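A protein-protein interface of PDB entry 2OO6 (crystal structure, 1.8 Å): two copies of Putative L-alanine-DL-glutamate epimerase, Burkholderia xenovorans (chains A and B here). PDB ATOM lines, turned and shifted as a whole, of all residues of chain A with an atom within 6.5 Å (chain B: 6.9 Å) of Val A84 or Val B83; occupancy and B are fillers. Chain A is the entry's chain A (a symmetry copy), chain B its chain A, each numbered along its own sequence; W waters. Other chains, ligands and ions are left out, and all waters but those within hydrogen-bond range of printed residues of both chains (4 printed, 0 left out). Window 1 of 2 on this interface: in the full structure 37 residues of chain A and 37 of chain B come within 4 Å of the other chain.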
ATOM      1  N   PRO A  44      -1.014 -14.347 -23.556  1.00  0.00           N
ATOM      2  CA  PRO A  44       0.294 -14.426 -24.231  1.00  0.00           C
ATOM      3  C   PRO A  44       0.981 -13.072 -24.060  1.00  0.00           C
ATOM      4  O   PRO A  44       0.284 -12.044 -24.046  1.00  0.00           O
ATOM      5  CB  PRO A  44      -0.079 -14.599 -25.717  1.00  0.00           C
ATOM      6  CG  PRO A  44      -1.485 -14.009 -25.845  1.00  0.00           C
ATOM      7  CD  PRO A  44      -2.140 -14.322 -24.520  1.00  0.00           C
ATOM      8  N   GLY A  45       2.313 -13.058 -23.936  1.00  0.00           N
ATOM      9  CA  GLY A  45       3.061 -11.805 -23.858  1.00  0.00           C
ATOM     10  C   GLY A  45       3.559 -11.416 -22.474  1.00  0.00           C
ATOM     11  O   GLY A  45       4.373 -10.503 -22.361  1.00  0.00           O
ATOM     12  N   VAL A  46       3.063 -12.066 -21.408  1.00  0.00           N
ATOM     13  CA  VAL A  46       3.456 -11.649 -20.054  1.00  0.00           C
ATOM     14  C   VAL A  46       4.990 -11.739 -19.843  1.00  0.00           C
ATOM     15  O   VAL A  46       5.589 -10.827 -19.296  1.00  0.00           O
ATOM     16  CB  VAL A  46       2.713 -12.420 -18.910  1.00  0.00           C
ATOM     17  CG1 VAL A  46       3.141 -11.897 -17.554  1.00  0.00           C
ATOM     18  CG2 VAL A  46       1.188 -12.303 -19.049  1.00  0.00           C
ATOM     19  N   VAL A  49       6.683  -8.771 -21.275  1.00  0.00           N
ATOM     20  CA  VAL A  49       6.502  -7.584 -20.457  1.00  0.00           C
ATOM     21  C   VAL A  49       7.513  -7.603 -19.304  1.00  0.00           C
ATOM     22  O   VAL A  49       8.191  -6.599 -19.043  1.00  0.00           O
ATOM     23  CB  VAL A  49       5.042  -7.476 -19.883  1.00  0.00           C
ATOM     24  CG1 VAL A  49       4.930  -6.287 -18.901  1.00  0.00           C
ATOM     25  CG2 VAL A  49       3.998  -7.347 -21.015  1.00  0.00           C
ATOM     26  N   LEU A  53      10.407  -4.786 -18.500  1.00  0.00           N
ATOM     27  CA  LEU A  53      10.324  -4.040 -17.256  1.00  0.00           C
ATOM     28  C   LEU A  53      11.444  -4.361 -16.268  1.00  0.00           C
ATOM     29  O   LEU A  53      11.924  -3.469 -15.553  1.00  0.00           O
ATOM     30  CB  LEU A  53       8.949  -4.241 -16.595  1.00  0.00           C
ATOM     31  CG  LEU A  53       7.792  -3.487 -17.276  1.00  0.00           C
ATOM     32  CD1 LEU A  53       6.488  -3.856 -16.561  1.00  0.00           C
ATOM     33  CD2 LEU A  53       8.003  -1.965 -17.263  1.00  0.00           C
ATOM     34  N   ALA A  72       6.765   1.747 -13.411  1.00  0.00           N
ATOM     35  CA  ALA A  72       6.321   0.814 -14.448  1.00  0.00           C
ATOM     36  C   ALA A  72       4.952   1.265 -15.002  1.00  0.00           C
ATOM     37  O   ALA A  72       4.719   1.277 -16.219  1.00  0.00           O
ATOM     38  CB  ALA A  72       6.241  -0.594 -13.885  1.00  0.00           C
ATOM     39  N   THR A  76       4.293   2.222 -19.010  1.00  0.00           N
ATOM     40  CA  THR A  76       3.347   1.427 -19.799  1.00  0.00           C
ATOM     41  C   THR A  76       1.914   1.999 -19.759  1.00  0.00           C
ATOM     42  O   THR A  76       0.973   1.310 -20.148  1.00  0.00           O
ATOM     43  CB  THR A  76       3.314  -0.062 -19.337  1.00  0.00           C
ATOM     44  OG1 THR A  76       2.924  -0.125 -17.960  1.00  0.00           O
ATOM     45  CG2 THR A  76       4.686  -0.734 -19.495  1.00  0.00           C
ATOM     46  N   ARG A  77       1.770   3.244 -19.295  1.00  0.00           N
ATOM     47  CA  ARG A  77       0.446   3.858 -19.073  1.00  0.00           C
ATOM     48  C   ARG A  77      -0.564   3.633 -20.211  1.00  0.00           C
ATOM     49  O   ARG A  77      -1.687   3.224 -19.938  1.00  0.00           O
ATOM     50  CB  ARG A  77       0.603   5.365 -18.808  1.00  0.00           C
ATOM     51  CG  ARG A  77      -0.144   5.817 -17.571  1.00  0.00           C
ATOM     52  CD  ARG A  77      -0.125   7.343 -17.460  1.00  0.00           C
ATOM     53  NE  ARG A  77      -0.720   7.725 -16.175  1.00  0.00           N
ATOM     54  CZ  ARG A  77      -0.040   8.008 -15.065  1.00  0.00           C
ATOM     55  NH1 ARG A  77      -0.713   8.305 -13.962  1.00  0.00           N
ATOM     56  NH2 ARG A  77       1.300   8.019 -15.050  1.00  0.00           N
ATOM     57  N   ALA A  79      -1.001   1.327 -22.481  1.00  0.00           N
ATOM     58  CA  ALA A  79      -1.488  -0.031 -22.693  1.00  0.00           C
ATOM     59  C   ALA A  79      -1.632  -0.787 -21.371  1.00  0.00           C
ATOM     60  O   ALA A  79      -1.458  -1.995 -21.302  1.00  0.00           O
ATOM     61  CB  ALA A  79      -0.561  -0.786 -23.687  1.00  0.00           C
ATOM     62  N   THR A  80      -1.974  -0.053 -20.317  1.00  0.00           N
ATOM     63  CA  THR A  80      -2.125  -0.632 -18.996  1.00  0.00           C
ATOM     64  C   THR A  80      -3.295  -1.637 -18.927  1.00  0.00           C
ATOM     65  O   THR A  80      -4.182  -1.680 -19.815  1.00  0.00           O
ATOM     66  CB  THR A  80      -2.245   0.470 -17.881  1.00  0.00           C
ATOM     67  OG1 THR A  80      -1.949  -0.109 -16.602  1.00  0.00           O
ATOM     68  CG2 THR A  80      -3.666   1.064 -17.843  1.00  0.00           C
ATOM     69  N   GLY A  81      -3.298  -2.434 -17.866  1.00  0.00           N
ATOM     70  CA  GLY A  81      -4.271  -3.515 -17.730  1.00  0.00           C
ATOM     71  C   GLY A  81      -3.774  -4.767 -18.418  1.00  0.00           C
ATOM     72  O   GLY A  81      -2.686  -4.768 -18.987  1.00  0.00           O
ATOM     73  N   GLY A  82      -4.554  -5.841 -18.337  1.00  0.00           N
ATOM     74  CA  GLY A  82      -4.264  -7.043 -19.109  1.00  0.00           C
ATOM     75  C   GLY A  82      -2.844  -7.533 -18.943  1.00  0.00           C
ATOM     76  O   GLY A  82      -2.306  -7.577 -17.825  1.00  0.00           O
ATOM     77  N   VAL A  83      -2.226  -7.864 -20.070  1.00  0.00           N
ATOM     78  CA  VAL A  83      -0.941  -8.557 -20.039  1.00  0.00           C
ATOM     79  C   VAL A  83       0.157  -7.658 -19.452  1.00  0.00           C
ATOM     80  O   VAL A  83       1.047  -8.122 -18.725  1.00  0.00           O
ATOM     81  CB  VAL A  83      -0.611  -9.124 -21.428  1.00  0.00           C
ATOM     82  CG1 VAL A  83       0.864  -9.354 -21.567  1.00  0.00           C
ATOM     83  CG2 VAL A  83      -1.388 -10.458 -21.625  1.00  0.00           C
ATOM     84  N   VAL A  84       0.059  -6.350 -19.706  1.00  0.00           N
ATOM     85  CA  VAL A  84       1.036  -5.422 -19.141  1.00  0.00           C
ATOM     86  C   VAL A  84       0.961  -5.462 -17.590  1.00  0.00           C
ATOM     87  O   VAL A  84       1.978  -5.607 -16.900  1.00  0.00           O
ATOM     88  CB  VAL A  84       0.823  -4.001 -19.710  1.00  0.00           C
ATOM     89  CG1 VAL A  84       1.437  -2.925 -18.795  1.00  0.00           C
ATOM     90  CG2 VAL A  84       1.411  -3.898 -21.139  1.00  0.00           C
ATOM     91  N   SER A  85      -0.250  -5.364 -17.044  1.00  0.00           N
ATOM     92  CA  SER A  85      -0.438  -5.295 -15.594  1.00  0.00           C
ATOM     93  C   SER A  85      -0.088  -6.627 -14.940  1.00  0.00           C
ATOM     94  O   SER A  85       0.392  -6.652 -13.804  1.00  0.00           O
ATOM     95  CB  SER A  85      -1.873  -4.861 -15.262  1.00  0.00           C
ATOM     96  OG  SER A  85      -2.034  -3.446 -15.520  1.00  0.00           O
ATOM     97  N   GLU A  86      -0.296  -7.727 -15.671  1.00  0.00           N
ATOM     98  CA  GLU A  86       0.144  -9.047 -15.206  1.00  0.00           C
ATOM     99  C   GLU A  86       1.660  -9.074 -15.047  1.00  0.00           C
ATOM    100  O   GLU A  86       2.183  -9.642 -14.072  1.00  0.00           O
ATOM    101  CB  GLU A  86      -0.278 -10.139 -16.202  1.00  0.00           C
ATOM    102  CG  GLU A  86      -1.761 -10.547 -16.084  1.00  0.00           C
ATOM    103  CD  GLU A  86      -2.121 -11.691 -17.010  1.00  0.00           C
ATOM    104  OE1 GLU A  86      -1.529 -12.762 -16.856  1.00  0.00           O
ATOM    105  OE2 GLU A  86      -3.019 -11.526 -17.873  1.00  0.00           O
ATOM    106  N   GLY A  87       2.363  -8.498 -16.021  1.00  0.00           N
ATOM    107  CA  GLY A  87       3.843  -8.409 -15.943  1.00  0.00           C
ATOM    108  C   GLY A  87       4.266  -7.617 -14.704  1.00  0.00           C
ATOM    109  O   GLY A  87       5.156  -8.022 -13.944  1.00  0.00           O
ATOM    110  N   ILE A  88       3.614  -6.475 -14.493  1.00  0.00           N
ATOM    111  CA  ILE A  88       3.903  -5.622 -13.335  1.00  0.00           C
ATOM    112  C   ILE A  88       3.652  -6.372 -12.024  1.00  0.00           C
ATOM    113  O   ILE A  88       4.478  -6.306 -11.078  1.00  0.00           O
ATOM    114  CB  ILE A  88       3.096  -4.273 -13.401  1.00  0.00           C
ATOM    115  CG1 ILE A  88       3.597  -3.449 -14.623  1.00  0.00           C
ATOM    116  CG2 ILE A  88       3.309  -3.468 -12.123  1.00  0.00           C
ATOM    117  CD1 ILE A  88       2.707  -2.188 -14.970  1.00  0.00           C
ATOM    118  N   GLY A  89       2.519  -7.062 -11.978  1.00  0.00           N
ATOM    119  CA  GLY A  89       2.088  -7.815 -10.797  1.00  0.00           C
ATOM    120  C   GLY A  89       3.069  -8.916 -10.428  1.00  0.00           C
ATOM    121  O   GLY A  89       3.371  -9.113  -9.247  1.00  0.00           O
ATOM    122  N   PHE A 272      -8.315  -5.560 -12.956  1.00  0.00           N
ATOM    123  CA  PHE A 272      -7.060  -4.960 -12.477  1.00  0.00           C
ATOM    124  C   PHE A 272      -7.262  -3.604 -11.800  1.00  0.00           C
ATOM    125  O   PHE A 272      -7.709  -2.644 -12.438  1.00  0.00           O
ATOM    126  CB  PHE A 272      -6.107  -4.718 -13.645  1.00  0.00           C
ATOM    127  CG  PHE A 272      -5.681  -5.964 -14.354  1.00  0.00           C
ATOM    128  CD1 PHE A 272      -4.466  -6.577 -14.032  1.00  0.00           C
ATOM    129  CD2 PHE A 272      -6.464  -6.510 -15.358  1.00  0.00           C
ATOM    130  CE1 PHE A 272      -4.052  -7.735 -14.694  1.00  0.00           C
ATOM    131  CE2 PHE A 272      -6.056  -7.680 -16.028  1.00  0.00           C
ATOM    132  CZ  PHE A 272      -4.845  -8.294 -15.687  1.00  0.00           C
ATOM    133  N   ASP B  38       2.997  -1.365 -33.159  1.00  0.00           N
ATOM    134  CA  ASP B  38       4.031  -0.723 -32.383  1.00  0.00           C
ATOM    135  C   ASP B  38       4.136  -1.360 -31.020  1.00  0.00           C
ATOM    136  O   ASP B  38       3.111  -1.754 -30.451  1.00  0.00           O
ATOM    137  CB  ASP B  38       3.699   0.757 -32.251  1.00  0.00           C
ATOM    138  CG  ASP B  38       4.520   1.453 -31.175  1.00  0.00           C
ATOM    139  OD1 ASP B  38       5.591   2.000 -31.537  1.00  0.00           O
ATOM    140  OD2 ASP B  38       4.083   1.455 -29.984  1.00  0.00           O
ATOM    141  N   GLU B  39       5.367  -1.475 -30.517  1.00  0.00           N
ATOM    142  CA  GLU B  39       5.603  -1.849 -29.120  1.00  0.00           C
ATOM    143  C   GLU B  39       6.096  -0.697 -28.223  1.00  0.00           C
ATOM    144  O   GLU B  39       5.935  -0.756 -26.993  1.00  0.00           O
ATOM    145  CB  GLU B  39       6.564  -3.031 -29.013  1.00  0.00           C
ATOM    146  CG  GLU B  39       5.988  -4.299 -29.586  1.00  0.00           C
ATOM    147  CD  GLU B  39       6.688  -5.551 -29.108  1.00  0.00           C
ATOM    148  OE1 GLU B  39       7.497  -5.489 -28.154  1.00  0.00           O
ATOM    149  OE2 GLU B  39       6.389  -6.617 -29.671  1.00  0.00           O
ATOM    150  N   GLY B  42       4.501   2.158 -24.870  1.00  0.00           N
ATOM    151  CA  GLY B  42       4.117   1.449 -23.636  1.00  0.00           C
ATOM    152  C   GLY B  42       3.569   0.044 -23.826  1.00  0.00           C
ATOM    153  O   GLY B  42       2.859  -0.465 -22.933  1.00  0.00           O
ATOM    154  N   SER B  43       3.940  -0.609 -24.939  1.00  0.00           N
ATOM    155  CA  SER B  43       3.277  -1.860 -25.341  1.00  0.00           C
ATOM    156  C   SER B  43       4.216  -3.054 -25.592  1.00  0.00           C
ATOM    157  O   SER B  43       4.153  -3.659 -26.677  1.00  0.00           O
ATOM    158  CB  SER B  43       2.363  -1.610 -26.571  1.00  0.00           C
ATOM    159  OG  SER B  43       1.406  -0.553 -26.339  1.00  0.00           O
ATOM    160  N   PRO B  44       5.034  -3.453 -24.583  1.00  0.00           N
ATOM    161  CA  PRO B  44       5.875  -4.649 -24.773  1.00  0.00           C
ATOM    162  C   PRO B  44       4.943  -5.857 -24.846  1.00  0.00           C
ATOM    163  O   PRO B  44       3.907  -5.857 -24.162  1.00  0.00           O
ATOM    164  CB  PRO B  44       6.682  -4.733 -23.463  1.00  0.00           C
ATOM    165  CG  PRO B  44       5.837  -3.988 -22.427  1.00  0.00           C
ATOM    166  CD  PRO B  44       5.167  -2.889 -23.218  1.00  0.00           C
ATOM    167  N   GLY B  45       5.294  -6.869 -25.648  1.00  0.00           N
ATOM    168  CA  GLY B  45       4.510  -8.102 -25.712  1.00  0.00           C
ATOM    169  C   GLY B  45       3.628  -8.262 -26.941  1.00  0.00           C
ATOM    170  O   GLY B  45       3.114  -9.354 -27.175  1.00  0.00           O
ATOM    171  N   VAL B  46       3.410  -7.189 -27.720  1.00  0.00           N
ATOM    172  CA  VAL B  46       2.489  -7.292 -28.860  1.00  0.00           C
ATOM    173  C   VAL B  46       2.939  -8.380 -29.871  1.00  0.00           C
ATOM    174  O   VAL B  46       2.126  -9.164 -30.332  1.00  0.00           O
ATOM    175  CB  VAL B  46       2.246  -5.936 -29.607  1.00  0.00           C
ATOM    176  CG1 VAL B  46       1.252  -6.124 -30.735  1.00  0.00           C
ATOM    177  CG2 VAL B  46       1.739  -4.848 -28.649  1.00  0.00           C
ATOM    178  N   THR B  47       4.234  -8.434 -30.177  1.00  0.00           N
ATOM    179  CA  THR B  47       4.742  -9.459 -31.085  1.00  0.00           C
ATOM    180  C   THR B  47       4.397 -10.858 -30.568  1.00  0.00           C
ATOM    181  O   THR B  47       3.932 -11.710 -31.331  1.00  0.00           O
ATOM    182  CB  THR B  47       6.265  -9.336 -31.304  1.00  0.00           C
ATOM    183  OG1 THR B  47       6.571  -8.045 -31.847  1.00  0.00           O
ATOM    184  CG2 THR B  47       6.756 -10.404 -32.241  1.00  0.00           C
ATOM    185  N   ALA B  48       4.603 -11.089 -29.269  1.00  0.00           N
ATOM    186  CA  ALA B  48       4.267 -12.376 -28.663  1.00  0.00           C
ATOM    187  C   ALA B  48       2.798 -12.738 -28.863  1.00  0.00           C
ATOM    188  O   ALA B  48       2.459 -13.891 -29.137  1.00  0.00           O
ATOM    189  CB  ALA B  48       4.616 -12.372 -27.142  1.00  0.00           C
ATOM    190  N   VAL B  49       1.919 -11.747 -28.711  1.00  0.00           N
ATOM    191  CA  VAL B  49       0.496 -11.982 -28.882  1.00  0.00           C
ATOM    192  C   VAL B  49       0.221 -12.400 -30.332  1.00  0.00           C
ATOM    193  O   VAL B  49      -0.486 -13.386 -30.581  1.00  0.00           O
ATOM    194  CB  VAL B  49      -0.362 -10.716 -28.521  1.00  0.00           C
ATOM    195  CG1 VAL B  49      -1.852 -10.954 -28.858  1.00  0.00           C
ATOM    196  CG2 VAL B  49      -0.195 -10.324 -27.035  1.00  0.00           C
ATOM    197  N   ILE B  50       0.782 -11.641 -31.278  1.00  0.00           N
ATOM    198  CA  ILE B  50       0.558 -11.924 -32.693  1.00  0.00           C
ATOM    199  C   ILE B  50       1.091 -13.329 -33.067  1.00  0.00           C
ATOM    200  O   ILE B  50       0.413 -14.093 -33.781  1.00  0.00           O
ATOM    201  CB  ILE B  50       1.207 -10.857 -33.576  1.00  0.00           C
ATOM    202  CG1 ILE B  50       0.482  -9.518 -33.388  1.00  0.00           C
ATOM    203  CG2 ILE B  50       1.173 -11.262 -35.069  1.00  0.00           C
ATOM    204  CD1 ILE B  50       1.324  -8.365 -33.865  1.00  0.00           C
ATOM    205  N   ALA B  79      -7.813 -11.515 -20.483  1.00  0.00           N
ATOM    206  CA  ALA B  79      -6.792 -10.473 -20.486  1.00  0.00           C
ATOM    207  C   ALA B  79      -6.950  -9.539 -21.687  1.00  0.00           C
ATOM    208  O   ALA B  79      -5.984  -9.006 -22.215  1.00  0.00           O
ATOM    209  CB  ALA B  79      -5.375 -11.109 -20.438  1.00  0.00           C
ATOM    210  N   THR B  80      -8.195  -9.330 -22.100  1.00  0.00           N
ATOM    211  CA  THR B  80      -8.493  -8.485 -23.240  1.00  0.00           C
ATOM    212  C   THR B  80      -8.119  -7.008 -22.989  1.00  0.00           C
ATOM    213  O   THR B  80      -7.897  -6.570 -21.833  1.00  0.00           O
ATOM    214  CB  THR B  80      -9.990  -8.629 -23.704  1.00  0.00           C
ATOM    215  OG1 THR B  80     -10.122  -8.147 -25.049  1.00  0.00           O
ATOM    216  CG2 THR B  80     -10.931  -7.821 -22.790  1.00  0.00           C
ATOM    217  N   GLY B  81      -8.061  -6.244 -24.072  1.00  0.00           N
ATOM    218  CA  GLY B  81      -7.598  -4.860 -24.003  1.00  0.00           C
ATOM    219  C   GLY B  81      -6.091  -4.796 -24.122  1.00  0.00           C
ATOM    220  O   GLY B  81      -5.438  -5.828 -24.255  1.00  0.00           O
ATOM    221  N   GLY B  82      -5.543  -3.585 -24.110  1.00  0.00           N
ATOM    222  CA  GLY B  82      -4.098  -3.413 -24.037  1.00  0.00           C
ATOM    223  C   GLY B  82      -3.347  -4.210 -25.079  1.00  0.00           C
ATOM    224  O   GLY B  82      -3.735  -4.255 -26.257  1.00  0.00           O
ATOM    225  N   VAL B  83      -2.289  -4.873 -24.628  1.00  0.00           N
ATOM    226  CA  VAL B  83      -1.351  -5.499 -25.555  1.00  0.00           C
ATOM    227  C   VAL B  83      -2.016  -6.655 -26.316  1.00  0.00           C
ATOM    228  O   VAL B  83      -1.754  -6.874 -27.507  1.00  0.00           O
ATOM    229  CB  VAL B  83      -0.062  -5.892 -24.819  1.00  0.00           C
ATOM    230  CG1 VAL B  83       0.665  -6.969 -25.567  1.00  0.00           C
ATOM    231  CG2 VAL B  83       0.840  -4.632 -24.672  1.00  0.00           C
ATOM    232  N   VAL B  84      -2.936  -7.359 -25.651  1.00  0.00           N
ATOM    233  CA  VAL B  84      -3.651  -8.442 -26.322  1.00  0.00           C
ATOM    234  C   VAL B  84      -4.469  -7.873 -27.513  1.00  0.00           C
ATOM    235  O   VAL B  84      -4.397  -8.373 -28.642  1.00  0.00           O
ATOM    236  CB  VAL B  84      -4.529  -9.216 -25.314  1.00  0.00           C
ATOM    237  CG1 VAL B  84      -5.662  -9.984 -26.019  1.00  0.00           C
ATOM    238  CG2 VAL B  84      -3.661 -10.183 -24.472  1.00  0.00           C
ATOM    239  N   SER B  85      -5.226  -6.804 -27.266  1.00  0.00           N
ATOM    240  CA  SER B  85      -6.112  -6.236 -28.283  1.00  0.00           C
ATOM    241  C   SER B  85      -5.303  -5.590 -29.404  1.00  0.00           C
ATOM    242  O   SER B  85      -5.736  -5.594 -30.559  1.00  0.00           O
ATOM    243  CB  SER B  85      -7.089  -5.238 -27.643  1.00  0.00           C
ATOM    244  OG  SER B  85      -8.111  -5.951 -26.907  1.00  0.00           O
ATOM    245  N   GLU B  86      -4.120  -5.069 -29.067  1.00  0.00           N
ATOM    246  CA  GLU B  86      -3.193  -4.560 -30.083  1.00  0.00           C
ATOM    247  C   GLU B  86      -2.770  -5.683 -31.023  1.00  0.00           C
ATOM    248  O   GLU B  86      -2.676  -5.481 -32.247  1.00  0.00           O
ATOM    249  CB  GLU B  86      -1.942  -3.959 -29.420  1.00  0.00           C
ATOM    250  CG  GLU B  86      -2.161  -2.542 -28.852  1.00  0.00           C
ATOM    251  CD  GLU B  86      -0.887  -1.940 -28.295  1.00  0.00           C
ATOM    252  OE1 GLU B  86       0.059  -1.782 -29.069  1.00  0.00           O
ATOM    253  OE2 GLU B  86      -0.845  -1.598 -27.087  1.00  0.00           O
ATOM    254  N   GLY B  87      -2.477  -6.850 -30.450  1.00  0.00           N
ATOM    255  CA  GLY B  87      -2.114  -8.032 -31.272  1.00  0.00           C
ATOM    256  C   GLY B  87      -3.258  -8.396 -32.220  1.00  0.00           C
ATOM    257  O   GLY B  87      -3.060  -8.637 -33.419  1.00  0.00           O
ATOM    258  N   ILE B  88      -4.474  -8.430 -31.678  1.00  0.00           N
ATOM    259  CA  ILE B  88      -5.666  -8.748 -32.471  1.00  0.00           C
ATOM    260  C   ILE B  88      -5.858  -7.735 -33.605  1.00  0.00           C
ATOM    261  O   ILE B  88      -6.148  -8.119 -34.766  1.00  0.00           O
ATOM    262  CB  ILE B  88      -6.946  -8.858 -31.564  1.00  0.00           C
ATOM    263  CG1 ILE B  88      -6.781 -10.077 -30.611  1.00  0.00           C
ATOM    264  CG2 ILE B  88      -8.190  -9.053 -32.427  1.00  0.00           C
ATOM    265  CD1 ILE B  88      -7.869 -10.165 -29.466  1.00  0.00           C
ATOM    266  N   PHE B 272      -9.834   0.910 -26.244  1.00  0.00           N
ATOM    267  CA  PHE B 272     -10.158  -0.243 -27.099  1.00  0.00           C
ATOM    268  C   PHE B 272     -11.645  -0.597 -27.096  1.00  0.00           C
ATOM    269  O   PHE B 272     -12.200  -0.962 -26.053  1.00  0.00           O
ATOM    270  CB  PHE B 272      -9.419  -1.488 -26.613  1.00  0.00           C
ATOM    271  CG  PHE B 272      -7.929  -1.378 -26.677  1.00  0.00           C
ATOM    272  CD1 PHE B 272      -7.231  -1.901 -27.769  1.00  0.00           C
ATOM    273  CD2 PHE B 272      -7.217  -0.790 -25.643  1.00  0.00           C
ATOM    274  CE1 PHE B 272      -5.839  -1.814 -27.836  1.00  0.00           C
ATOM    275  CE2 PHE B 272      -5.815  -0.695 -25.704  1.00  0.00           C
ATOM    276  CZ  PHE B 272      -5.126  -1.207 -26.810  1.00  0.00           C
HETATM  277  O   HOH W   1      -1.760  -4.736 -21.825  1.00  0.00           O
HETATM  278  O   HOH W   2      -3.656  -7.468 -22.509  1.00  0.00           O
HETATM  279  O   HOH W   3      -7.619  -7.241 -19.254  1.00  0.00           O
HETATM  280  O   HOH W   4      -4.941  -0.725 -22.200  1.00  0.00           O
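The side-chain hydroxyl (OG) of Ser B43 sits at hydrogen-bond distance from the side-chain carboxylate (OE2) of Glu B86, at 2.6 Å.
The side-chain hydroxyl of Thr A76 lies within hydrogen-bond range of the backbone carbonyl oxygen of Ala A72.
Among the printed residues, pairs that only touch across the chains: Pro A44 with Val B49 (3.5 Å), Gly A45 with Ala B48 (3.7 Å), Val A49 with Pro B44 (3.5 Å), Thr A76 with Gly B42 (3.6 Å), Ala A79 with Gly B42 (3.5 Å), Ala A79 with Ser B43 (3.3 Å), Ala A79 with Glu B86 (3.5 Å), Val A83 with Val B84 (3.7 Å), Val A84 with Val B83 (3.7 Å) and Glu A86 with Ala B79 (3.5 Å).
Printed residues of chain B within 4 Å of Gly A45: Ala B48 (3.7 Å).
Ala A72 touches none of the printed residues of chain B.
Printed residues of chain B within 4 Å of Thr A76: Gly B42.
Gly A81 touches none of the printed residues of chain B.
Printed residues of chain B within 4 Å of Val A84: Val B83.
Of the printed residues of chain A, Gly B42 touches Thr A76 and Ala A79.
Of the printed residues of chain A, Ala B48 touches Gly A45.
Val B83 touches just one residue of chain A: Val A84 (3.7 Å).
Hydrophobic or aromatic side chains of chain B that line the printed part of chain A: Ala B48, Val B49, Ala B79, Val B83 and Val B84.
Of the 20 printed residues of chain A, 8 touch a printed residue of chain B.
Printed residues of chain A that touch a printed residue of chain B: Pro A44, Gly A45, Val A49, Thr A76, Ala A79, Val A83, Val A84 and Glu A86.
Among the printed residues, 10 pairs touch across the chains.
Pro A44 touches Val B49, and with the chains exchanged Val A49 touches Pro B44.
Ala A79 touches Glu B86, and with the chains exchanged Glu A86 touches Ala B79.
Val A83 touches Val B84, and with the chains exchanged Val A84 touches Val B83.
Of the 10 pairs that touch across the chains among the printed residues, 6 have their exchanged pair printed and touching as well.
Water W4 bridges the backbone carbonyl oxygen (O) of Thr A80 (2.7 Å) and the backbone NH (N) of Gly B82 (3.5 Å).
Water W3 lies within hydrogen-bond range of O of Thr B80 (2.7 Å) and N of Gly A82 (3.5 Å).
Water W1 lies within hydrogen-bond range of O of Ala A79 (2.8 Å), N of Val B83 (2.9 Å), O of Gly A81 (3.0 Å) and N of Val A84 (3.2 Å).
Water W2 lies within hydrogen-bond range of O of Ala B79 (2.8 Å), N of Val A83 (2.9 Å), O of Gly B81 (3.0 Å) and N of Val B84 (3.2 Å).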
